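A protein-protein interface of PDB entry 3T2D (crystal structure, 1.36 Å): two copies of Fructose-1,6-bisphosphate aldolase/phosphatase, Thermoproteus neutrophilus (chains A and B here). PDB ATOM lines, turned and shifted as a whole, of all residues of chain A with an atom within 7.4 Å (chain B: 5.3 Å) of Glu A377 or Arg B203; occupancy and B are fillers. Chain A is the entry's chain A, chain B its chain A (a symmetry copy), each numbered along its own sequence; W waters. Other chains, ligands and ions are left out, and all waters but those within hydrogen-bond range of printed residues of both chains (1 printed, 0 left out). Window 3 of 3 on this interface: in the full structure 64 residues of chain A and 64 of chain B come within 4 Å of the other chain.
Of the 12 printed residues of chain A, 5 touch a printed residue of chain B. Printed residues of chain B that touch a printed residue of chain A: Glu B169, Val B178, Arg B203 and Lys B204. Among the printed residues, 9 pairs touch across the chains. Among the printed residues, Asp or Glu carboxylates within 4 Å of a Lys or Arg side-chain nitrogen of the other chain: Glu A377 with Arg B203 (3.6 Å) and Arg A380 with Glu B169 (2.8 Å).
Among the printed residues, merely in contact across the chains: Arg A380 with Arg B203, Tyr A376 with Val B178, Tyr A376 with Arg B203, Ala A373 with Val B178 and Arg A380 with Lys B204.
OE2 of Glu A377 is in salt-bridge range of NH2 of Arg A380 (3.0 Å). NE of Arg B203 lies within salt-bridge range of OE1 of Glu B169, at 2.9 Å. The backbone NH of Glu B169 sits at hydrogen-bond distance from the backbone carbonyl oxygen of Lys B204 (2.8 Å). The backbone carbonyl oxygen (O) of Arg B203 sits at hydrogen-bond distance from the backbone NH (N) of Asn B217, at 2.8 Å.
Water W1 lies within hydrogen-bond range of OE2 of Glu A377 (2.7 Å), NH2 of Arg B203 (2.8 Å) and O of Ala A373 (2.8 Å).
No position is printed for both chains.
N of Val B178 is in hydrogen-bond range of O of Tyr A371, at 2.8 Å. OH of Tyr A376 lies within hydrogen-bond range of OE2 of Glu B169 (2.6 Å). NH2 of Arg B203 lies within salt-bridge range of OE2 of Glu A377 (3.6 Å). The side-chain carboxylate (OE2) of Glu B169 lies within salt-bridge range of the guanidinium group (NE) of Arg A380 (2.8 Å).
Of the printed residues of chain B, Tyr A371 touches Val B178 (2.8 Å). Printed residues of chain B within 4 Å of Ala A373: Val B178. Of the printed residues of chain B, Glu A377 touches Arg B203 (3.6 Å). Tyr A383 touches none of the printed residues of chain B. Of the printed residues of chain A, Glu B169 touches Tyr A376 and Arg A380. Of the printed residues of chain A, Val B178 touches Tyr A371 (2.8 Å), Ala A373 (3.95 Å) and Tyr A376 (3.8 Å). Of chain A, only Tyr A376, Glu A377 and Arg A380 come within 4 Å of Arg B203. Asn B217 touches none of the printed residues of chain A. The nearest residue of chain B that does not touch Glu A377 is Asp B65 (4.4 Å).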
ATOM      1  N   TYR A 371      20.525   8.595  26.266  1.00  0.00           N
ATOM      2  CA  TYR A 371      20.265   8.392  27.670  1.00  0.00           C
ATOM      3  C   TYR A 371      19.224   7.305  27.780  1.00  0.00           C
ATOM      4  O   TYR A 371      18.143   7.361  27.201  1.00  0.00           O
ATOM      5  CB  TYR A 371      19.743   9.651  28.350  1.00  0.00           C
ATOM      6  CG  TYR A 371      20.623  10.812  28.188  1.00  0.00           C
ATOM      7  CD1 TYR A 371      21.631  11.021  29.106  1.00  0.00           C
ATOM      8  CD2 TYR A 371      20.455  11.761  27.207  1.00  0.00           C
ATOM      9  CE1 TYR A 371      22.449  12.134  29.014  1.00  0.00           C
ATOM     10  CE2 TYR A 371      21.266  12.886  27.062  1.00  0.00           C
ATOM     11  CZ  TYR A 371      22.282  13.093  27.990  1.00  0.00           C
ATOM     12  OH  TYR A 371      23.082  14.207  27.900  1.00  0.00           O
ATOM     13  N   PRO A 372      19.526   6.207  28.505  1.00  0.00           N
ATOM     14  CA  PRO A 372      18.462   5.248  28.841  1.00  0.00           C
ATOM     15  C   PRO A 372      17.262   5.975  29.391  1.00  0.00           C
ATOM     16  O   PRO A 372      17.438   6.854  30.277  1.00  0.00           O
ATOM     17  CB  PRO A 372      19.127   4.321  29.887  1.00  0.00           C
ATOM     18  CG  PRO A 372      20.559   4.452  29.582  1.00  0.00           C
ATOM     19  CD  PRO A 372      20.852   5.844  29.114  1.00  0.00           C
ATOM     20  N   ALA A 373      16.077   5.672  28.885  1.00  0.00           N
ATOM     21  CA  ALA A 373      14.891   6.449  29.208  1.00  0.00           C
ATOM     22  C   ALA A 373      14.476   6.495  30.660  1.00  0.00           C
ATOM     23  O   ALA A 373      14.033   7.510  31.186  1.00  0.00           O
ATOM     24  CB  ALA A 373      13.697   6.060  28.286  1.00  0.00           C
ATOM     25  N   ASP A 374      14.670   5.410  31.372  1.00  0.00           N
ATOM     26  CA  ASP A 374      14.226   5.391  32.775  1.00  0.00           C
ATOM     27  C   ASP A 374      15.125   6.273  33.674  1.00  0.00           C
ATOM     28  O   ASP A 374      14.676   7.146  34.443  1.00  0.00           O
ATOM     29  CB  ASP A 374      14.228   3.954  33.226  1.00  0.00           C
ATOM     30  CG  ASP A 374      13.097   3.106  32.613  1.00  0.00           C
ATOM     31  OD1 ASP A 374      11.976   3.615  32.244  1.00  0.00           O
ATOM     32  OD2 ASP A 374      13.361   1.879  32.527  1.00  0.00           O
ATOM     33  N   GLN A 375      16.395   6.234  33.417  1.00  0.00           N
ATOM     34  CA  GLN A 375      17.281   7.077  34.152  1.00  0.00           C
ATOM     35  C   GLN A 375      17.207   8.507  33.733  1.00  0.00           C
ATOM     36  O   GLN A 375      17.307   9.434  34.566  1.00  0.00           O
ATOM     37  CB  GLN A 375      18.698   6.558  34.030  1.00  0.00           C
ATOM     38  CG  GLN A 375      19.716   7.251  34.978  1.00  0.00           C
ATOM     39  CD  GLN A 375      19.397   7.251  36.552  1.00  0.00           C
ATOM     40  OE1 GLN A 375      19.694   8.260  37.255  1.00  0.00           O
ATOM     41  NE2 GLN A 375      18.794   6.143  37.076  1.00  0.00           N
ATOM     42  N   TYR A 376      16.965   8.737  32.422  1.00  0.00           N
ATOM     43  CA  TYR A 376      16.732  10.103  31.961  1.00  0.00           C
ATOM     44  C   TYR A 376      15.605  10.806  32.731  1.00  0.00           C
ATOM     45  O   TYR A 376      15.794  11.969  33.051  1.00  0.00           O
ATOM     46  CB  TYR A 376      16.471  10.140  30.470  1.00  0.00           C
ATOM     47  CG  TYR A 376      16.170  11.549  29.934  1.00  0.00           C
ATOM     48  CD1 TYR A 376      14.864  12.037  29.874  1.00  0.00           C
ATOM     49  CD2 TYR A 376      17.172  12.360  29.540  1.00  0.00           C
ATOM     50  CE1 TYR A 376      14.639  13.304  29.428  1.00  0.00           C
ATOM     51  CE2 TYR A 376      16.942  13.667  29.109  1.00  0.00           C
ATOM     52  CZ  TYR A 376      15.608  14.125  29.073  1.00  0.00           C
ATOM     53  OH  TYR A 376      15.435  15.402  28.613  1.00  0.00           O
ATOM     54  N   GLU A 377      14.474  10.166  33.012  1.00  0.00           N
ATOM     55  CA  GLU A 377      13.451  10.843  33.783  1.00  0.00           C
ATOM     56  C   GLU A 377      13.939  11.477  35.075  1.00  0.00           C
ATOM     57  O   GLU A 377      13.549  12.595  35.428  1.00  0.00           O
ATOM     58  CB  GLU A 377      12.401   9.897  34.292  1.00  0.00           C
ATOM     59  CG  GLU A 377      11.405   9.538  33.304  1.00  0.00           C
ATOM     60  CD  GLU A 377      10.755  10.773  32.658  1.00  0.00           C
ATOM     61  OE1 GLU A 377      10.177  11.701  33.358  1.00  0.00           O
ATOM     62  OE2 GLU A 377      10.862  10.821  31.417  1.00  0.00           O
ATOM     63  N   LYS A 378      14.803  10.767  35.805  1.00  0.00           N
ATOM     64  CA  LYS A 378      15.334  11.374  37.058  1.00  0.00           C
ATOM     65  C   LYS A 378      16.281  12.547  36.824  1.00  0.00           C
ATOM     66  O   LYS A 378      16.386  13.467  37.632  1.00  0.00           O
ATOM     67  CB  LYS A 378      16.069  10.263  37.844  1.00  0.00           C
ATOM     68  CG  LYS A 378      15.179   9.054  38.082  1.00  0.00           C
ATOM     69  CD  LYS A 378      15.719   8.211  39.305  1.00  0.00           C
ATOM     70  CE  LYS A 378      15.172   6.724  39.349  1.00  0.00           C
ATOM     71  NZ  LYS A 378      15.958   5.789  38.426  1.00  0.00           N
ATOM     72  N   ASP A 379      17.004  12.538  35.719  1.00  0.00           N
ATOM     73  CA  ASP A 379      18.110  13.457  35.501  1.00  0.00           C
ATOM     74  C   ASP A 379      17.730  14.627  34.566  1.00  0.00           C
ATOM     75  O   ASP A 379      18.594  15.421  34.220  1.00  0.00           O
ATOM     76  CB  ASP A 379      19.321  12.695  34.890  1.00  0.00           C
ATOM     77  CG  ASP A 379      19.989  11.730  35.919  1.00  0.00           C
ATOM     78  OD1 ASP A 379      19.942  12.011  37.180  1.00  0.00           O
ATOM     79  OD2 ASP A 379      20.501  10.676  35.369  1.00  0.00           O
ATOM     80  N   ARG A 380      16.502  14.614  34.018  1.00  0.00           N
ATOM     81  CA  ARG A 380      16.111  15.571  32.945  1.00  0.00           C
ATOM     82  C   ARG A 380      16.379  17.007  33.286  1.00  0.00           C
ATOM     83  O   ARG A 380      17.105  17.727  32.548  1.00  0.00           O
ATOM     84  CB  ARG A 380      14.595  15.413  32.724  1.00  0.00           C
ATOM     85  CG  ARG A 380      14.076  16.508  31.775  1.00  0.00           C
ATOM     86  CD  ARG A 380      12.581  16.595  31.517  1.00  0.00           C
ATOM     87  NE  ARG A 380      12.084  15.522  30.679  1.00  0.00           N
ATOM     88  CZ  ARG A 380      11.479  14.468  31.090  1.00  0.00           C
ATOM     89  NH1 ARG A 380      11.401  14.258  32.463  1.00  0.00           N
ATOM     90  NH2 ARG A 380      11.018  13.538  30.277  1.00  0.00           N
ATOM     91  N   LYS A 381      15.966  17.425  34.474  1.00  0.00           N
ATOM     92  CA  LYS A 381      16.282  18.776  34.881  1.00  0.00           C
ATOM     93  C   LYS A 381      17.755  19.069  34.916  1.00  0.00           C
ATOM     94  O   LYS A 381      18.172  20.087  34.450  1.00  0.00           O
ATOM     95  CB  LYS A 381      15.648  19.131  36.216  1.00  0.00           C
ATOM     96  CG  LYS A 381      16.683  19.463  37.254  1.00  0.00           C
ATOM     97  CD  LYS A 381      17.352  18.173  37.781  1.00  0.00           C
ATOM     98  CE  LYS A 381      17.456  18.108  39.364  1.00  0.00           C
ATOM     99  NZ  LYS A 381      16.265  17.601  40.100  1.00  0.00           N
ATOM    100  N   TYR A 383      20.037  17.526  33.092  1.00  0.00           N
ATOM    101  CA  TYR A 383      20.543  17.581  31.750  1.00  0.00           C
ATOM    102  C   TYR A 383      20.155  18.827  30.994  1.00  0.00           C
ATOM    103  O   TYR A 383      20.984  19.453  30.276  1.00  0.00           O
ATOM    104  CB  TYR A 383      20.024  16.385  31.041  1.00  0.00           C
ATOM    105  CG  TYR A 383      20.626  15.117  31.439  1.00  0.00           C
ATOM    106  CD1 TYR A 383      21.947  15.055  31.917  1.00  0.00           C
ATOM    107  CD2 TYR A 383      19.832  14.007  31.533  1.00  0.00           C
ATOM    108  CE1 TYR A 383      22.472  13.859  32.260  1.00  0.00           C
ATOM    109  CE2 TYR A 383      20.308  12.832  31.859  1.00  0.00           C
ATOM    110  CZ  TYR A 383      21.643  12.731  32.273  1.00  0.00           C
ATOM    111  OH  TYR A 383      22.125  11.505  32.660  1.00  0.00           O
ATOM    112  N   ASP B  65       3.074  13.883  36.314  1.00  0.00           N
ATOM    113  CA  ASP B  65       3.120  12.494  36.718  1.00  0.00           C
ATOM    114  C   ASP B  65       2.474  12.335  38.072  1.00  0.00           C
ATOM    115  O   ASP B  65       2.917  11.480  38.898  1.00  0.00           O
ATOM    116  CB  ASP B  65       4.524  11.935  36.703  1.00  0.00           C
ATOM    117  CG  ASP B  65       5.131  11.914  35.333  1.00  0.00           C
ATOM    118  OD1 ASP B  65       4.466  11.316  34.470  1.00  0.00           O
ATOM    119  OD2 ASP B  65       6.214  12.536  35.172  1.00  0.00           O
ATOM    120  N   GLU B 169      13.784  17.101  23.099  1.00  0.00           N
ATOM    121  CA  GLU B 169      13.898  15.789  23.768  1.00  0.00           C
ATOM    122  C   GLU B 169      13.200  14.796  22.891  1.00  0.00           C
ATOM    123  O   GLU B 169      11.966  14.841  22.752  1.00  0.00           O
ATOM    124  CB  GLU B 169      13.263  15.876  25.133  1.00  0.00           C
ATOM    125  CG  GLU B 169      13.207  14.620  25.912  1.00  0.00           C
ATOM    126  CD  GLU B 169      12.492  14.721  27.232  1.00  0.00           C
ATOM    127  OE1 GLU B 169      11.617  13.885  27.475  1.00  0.00           O
ATOM    128  OE2 GLU B 169      12.874  15.662  27.986  1.00  0.00           O
ATOM    129  N   VAL B 170      13.988  13.914  22.283  1.00  0.00           N
ATOM    130  CA  VAL B 170      13.497  12.942  21.299  1.00  0.00           C
ATOM    131  C   VAL B 170      13.544  11.553  21.944  1.00  0.00           C
ATOM    132  O   VAL B 170      14.593  11.138  22.496  1.00  0.00           O
ATOM    133  CB  VAL B 170      14.412  12.960  20.049  1.00  0.00           C
ATOM    134  CG1 VAL B 170      14.003  11.836  19.082  1.00  0.00           C
ATOM    135  CG2 VAL B 170      14.345  14.341  19.393  1.00  0.00           C
ATOM    136  N   LEU B 171      12.433  10.829  21.916  1.00  0.00           N
ATOM    137  CA  LEU B 171      12.297   9.487  22.409  1.00  0.00           C
ATOM    138  C   LEU B 171      12.389   8.486  21.297  1.00  0.00           C
ATOM    139  O   LEU B 171      11.594   8.538  20.342  1.00  0.00           O
ATOM    140  CB  LEU B 171      11.006   9.345  23.196  1.00  0.00           C
ATOM    141  CG  LEU B 171      10.726   7.956  23.813  1.00  0.00           C
ATOM    142  CD1 LEU B 171      11.806   7.607  24.895  1.00  0.00           C
ATOM    143  CD2 LEU B 171       9.328   7.925  24.411  1.00  0.00           C
ATOM    144  N   VAL B 178      16.630   8.233  25.021  1.00  0.00           N
ATOM    145  CA  VAL B 178      16.318   9.636  24.894  1.00  0.00           C
ATOM    146  C   VAL B 178      17.538  10.350  24.313  1.00  0.00           C
ATOM    147  O   VAL B 178      18.693  10.127  24.716  1.00  0.00           O
ATOM    148  CB  VAL B 178      15.886  10.273  26.198  1.00  0.00           C
ATOM    149  CG1 VAL B 178      15.696  11.834  26.062  1.00  0.00           C
ATOM    150  CG2 VAL B 178      14.616   9.572  26.728  1.00  0.00           C
ATOM    151  N   ILE B 201      10.457  10.230  18.166  1.00  0.00           N
ATOM    152  CA  ILE B 201       9.357  11.147  18.314  1.00  0.00           C
ATOM    153  C   ILE B 201       9.754  12.272  19.245  1.00  0.00           C
ATOM    154  O   ILE B 201      10.312  12.042  20.349  1.00  0.00           O
ATOM    155  CB  ILE B 201       8.060  10.492  18.754  1.00  0.00           C
ATOM    156  CG1 ILE B 201       7.649   9.446  17.695  1.00  0.00           C
ATOM    157  CG2 ILE B 201       6.925  11.475  18.973  1.00  0.00           C
ATOM    158  CD1 ILE B 201       7.882   8.117  17.919  1.00  0.00           C
ATOM    159  N   ILE B 202       9.503  13.529  18.868  1.00  0.00           N
ATOM    160  CA  ILE B 202       9.687  14.658  19.777  1.00  0.00           C
ATOM    161  C   ILE B 202       8.720  14.533  20.904  1.00  0.00           C
ATOM    162  O   ILE B 202       7.517  14.560  20.713  1.00  0.00           O
ATOM    163  CB  ILE B 202       9.523  16.006  19.069  1.00  0.00           C
ATOM    164  CG1 ILE B 202      10.518  16.174  17.912  1.00  0.00           C
ATOM    165  CG2 ILE B 202       9.608  17.178  20.119  1.00  0.00           C
ATOM    166  CD1 ILE B 202      10.220  17.321  16.937  1.00  0.00           C
ATOM    167  N   ARG B 203       9.238  14.405  22.156  1.00  0.00           N
ATOM    168  CA  ARG B 203       8.405  14.322  23.309  1.00  0.00           C
ATOM    169  C   ARG B 203       8.274  15.682  24.063  1.00  0.00           C
ATOM    170  O   ARG B 203       7.163  15.985  24.540  1.00  0.00           O
ATOM    171  CB  ARG B 203       8.977  13.235  24.289  1.00  0.00           C
ATOM    172  CG  ARG B 203       8.075  13.018  25.483  1.00  0.00           C
ATOM    173  CD  ARG B 203       8.431  11.742  26.235  1.00  0.00           C
ATOM    174  NE  ARG B 203       9.781  11.802  26.788  1.00  0.00           N
ATOM    175  CZ  ARG B 203      10.381  10.831  27.496  1.00  0.00           C
ATOM    176  NH1 ARG B 203       9.736   9.691  27.669  1.00  0.00           N
ATOM    177  NH2 ARG B 203      11.610  11.022  27.909  1.00  0.00           N
ATOM    178  N   LYS B 204       9.364  16.400  24.154  1.00  0.00           N
ATOM    179  CA  LYS B 204       9.320  17.701  24.810  1.00  0.00           C
ATOM    180  C   LYS B 204      10.236  18.670  24.072  1.00  0.00           C
ATOM    181  O   LYS B 204      11.207  18.244  23.427  1.00  0.00           O
ATOM    182  CB  LYS B 204       9.677  17.579  26.338  1.00  0.00           C
ATOM    183  CG  LYS B 204       8.491  16.973  27.306  1.00  0.00           C
ATOM    184  CD  LYS B 204       8.854  16.751  28.674  1.00  0.00           C
ATOM    185  CE  LYS B 204       7.604  16.412  29.476  1.00  0.00           C
ATOM    186  NZ  LYS B 204       6.578  17.404  30.045  1.00  0.00           N
ATOM    187  N   VAL B 205       9.938  19.965  24.191  1.00  0.00           N
ATOM    188  CA  VAL B 205      10.811  21.001  23.676  1.00  0.00           C
ATOM    189  C   VAL B 205      11.011  22.029  24.805  1.00  0.00           C
ATOM    190  O   VAL B 205      10.064  22.314  25.541  1.00  0.00           O
ATOM    191  CB  VAL B 205      10.222  21.711  22.445  1.00  0.00           C
ATOM    192  CG1 VAL B 205      11.169  22.796  21.901  1.00  0.00           C
ATOM    193  CG2 VAL B 205       9.901  20.679  21.348  1.00  0.00           C
ATOM    194  N   ALA B 215       6.922  22.883  24.834  1.00  0.00           N
ATOM    195  CA  ALA B 215       5.913  21.968  24.302  1.00  0.00           C
ATOM    196  C   ALA B 215       6.056  20.609  24.938  1.00  0.00           C
ATOM    197  O   ALA B 215       7.172  20.212  25.344  1.00  0.00           O
ATOM    198  CB  ALA B 215       6.051  21.817  22.764  1.00  0.00           C
ATOM    199  N   ALA B 216       4.959  19.875  24.976  1.00  0.00           N
ATOM    200  CA  ALA B 216       4.914  18.505  25.434  1.00  0.00           C
ATOM    201  C   ALA B 216       3.955  17.721  24.558  1.00  0.00           C
ATOM    202  O   ALA B 216       2.788  18.108  24.425  1.00  0.00           O
ATOM    203  CB  ALA B 216       4.438  18.459  26.922  1.00  0.00           C
ATOM    204  N   ASN B 217       4.466  16.649  23.958  1.00  0.00           N
ATOM    205  CA  ASN B 217       3.726  15.761  23.068  1.00  0.00           C
ATOM    206  C   ASN B 217       3.477  14.434  23.772  1.00  0.00           C
ATOM    207  O   ASN B 217       4.406  13.986  24.488  1.00  0.00           O
ATOM    208  CB  ASN B 217       4.578  15.522  21.823  1.00  0.00           C
ATOM    209  CG  ASN B 217       3.852  14.770  20.690  1.00  0.00           C
ATOM    210  OD1 ASN B 217       2.633  14.678  20.655  1.00  0.00           O
ATOM    211  ND2 ASN B 217       4.675  14.266  19.747  1.00  0.00           N
ATOM    212  N   VAL B 219       3.698  10.826  23.831  1.00  0.00           N
ATOM    213  CA  VAL B 219       4.328   9.654  23.218  1.00  0.00           C
ATOM    214  C   VAL B 219       4.901   8.786  24.319  1.00  0.00           C
ATOM    215  O   VAL B 219       5.512   9.298  25.251  1.00  0.00           O
ATOM    216  CB  VAL B 219       5.411  10.045  22.192  1.00  0.00           C
ATOM    217  CG1 VAL B 219       6.532  10.979  22.805  1.00  0.00           C
ATOM    218  CG2 VAL B 219       5.945   8.838  21.448  1.00  0.00           C
HETATM  219  O   HOH W   1      12.221   9.137  29.850  1.00  0.00           O
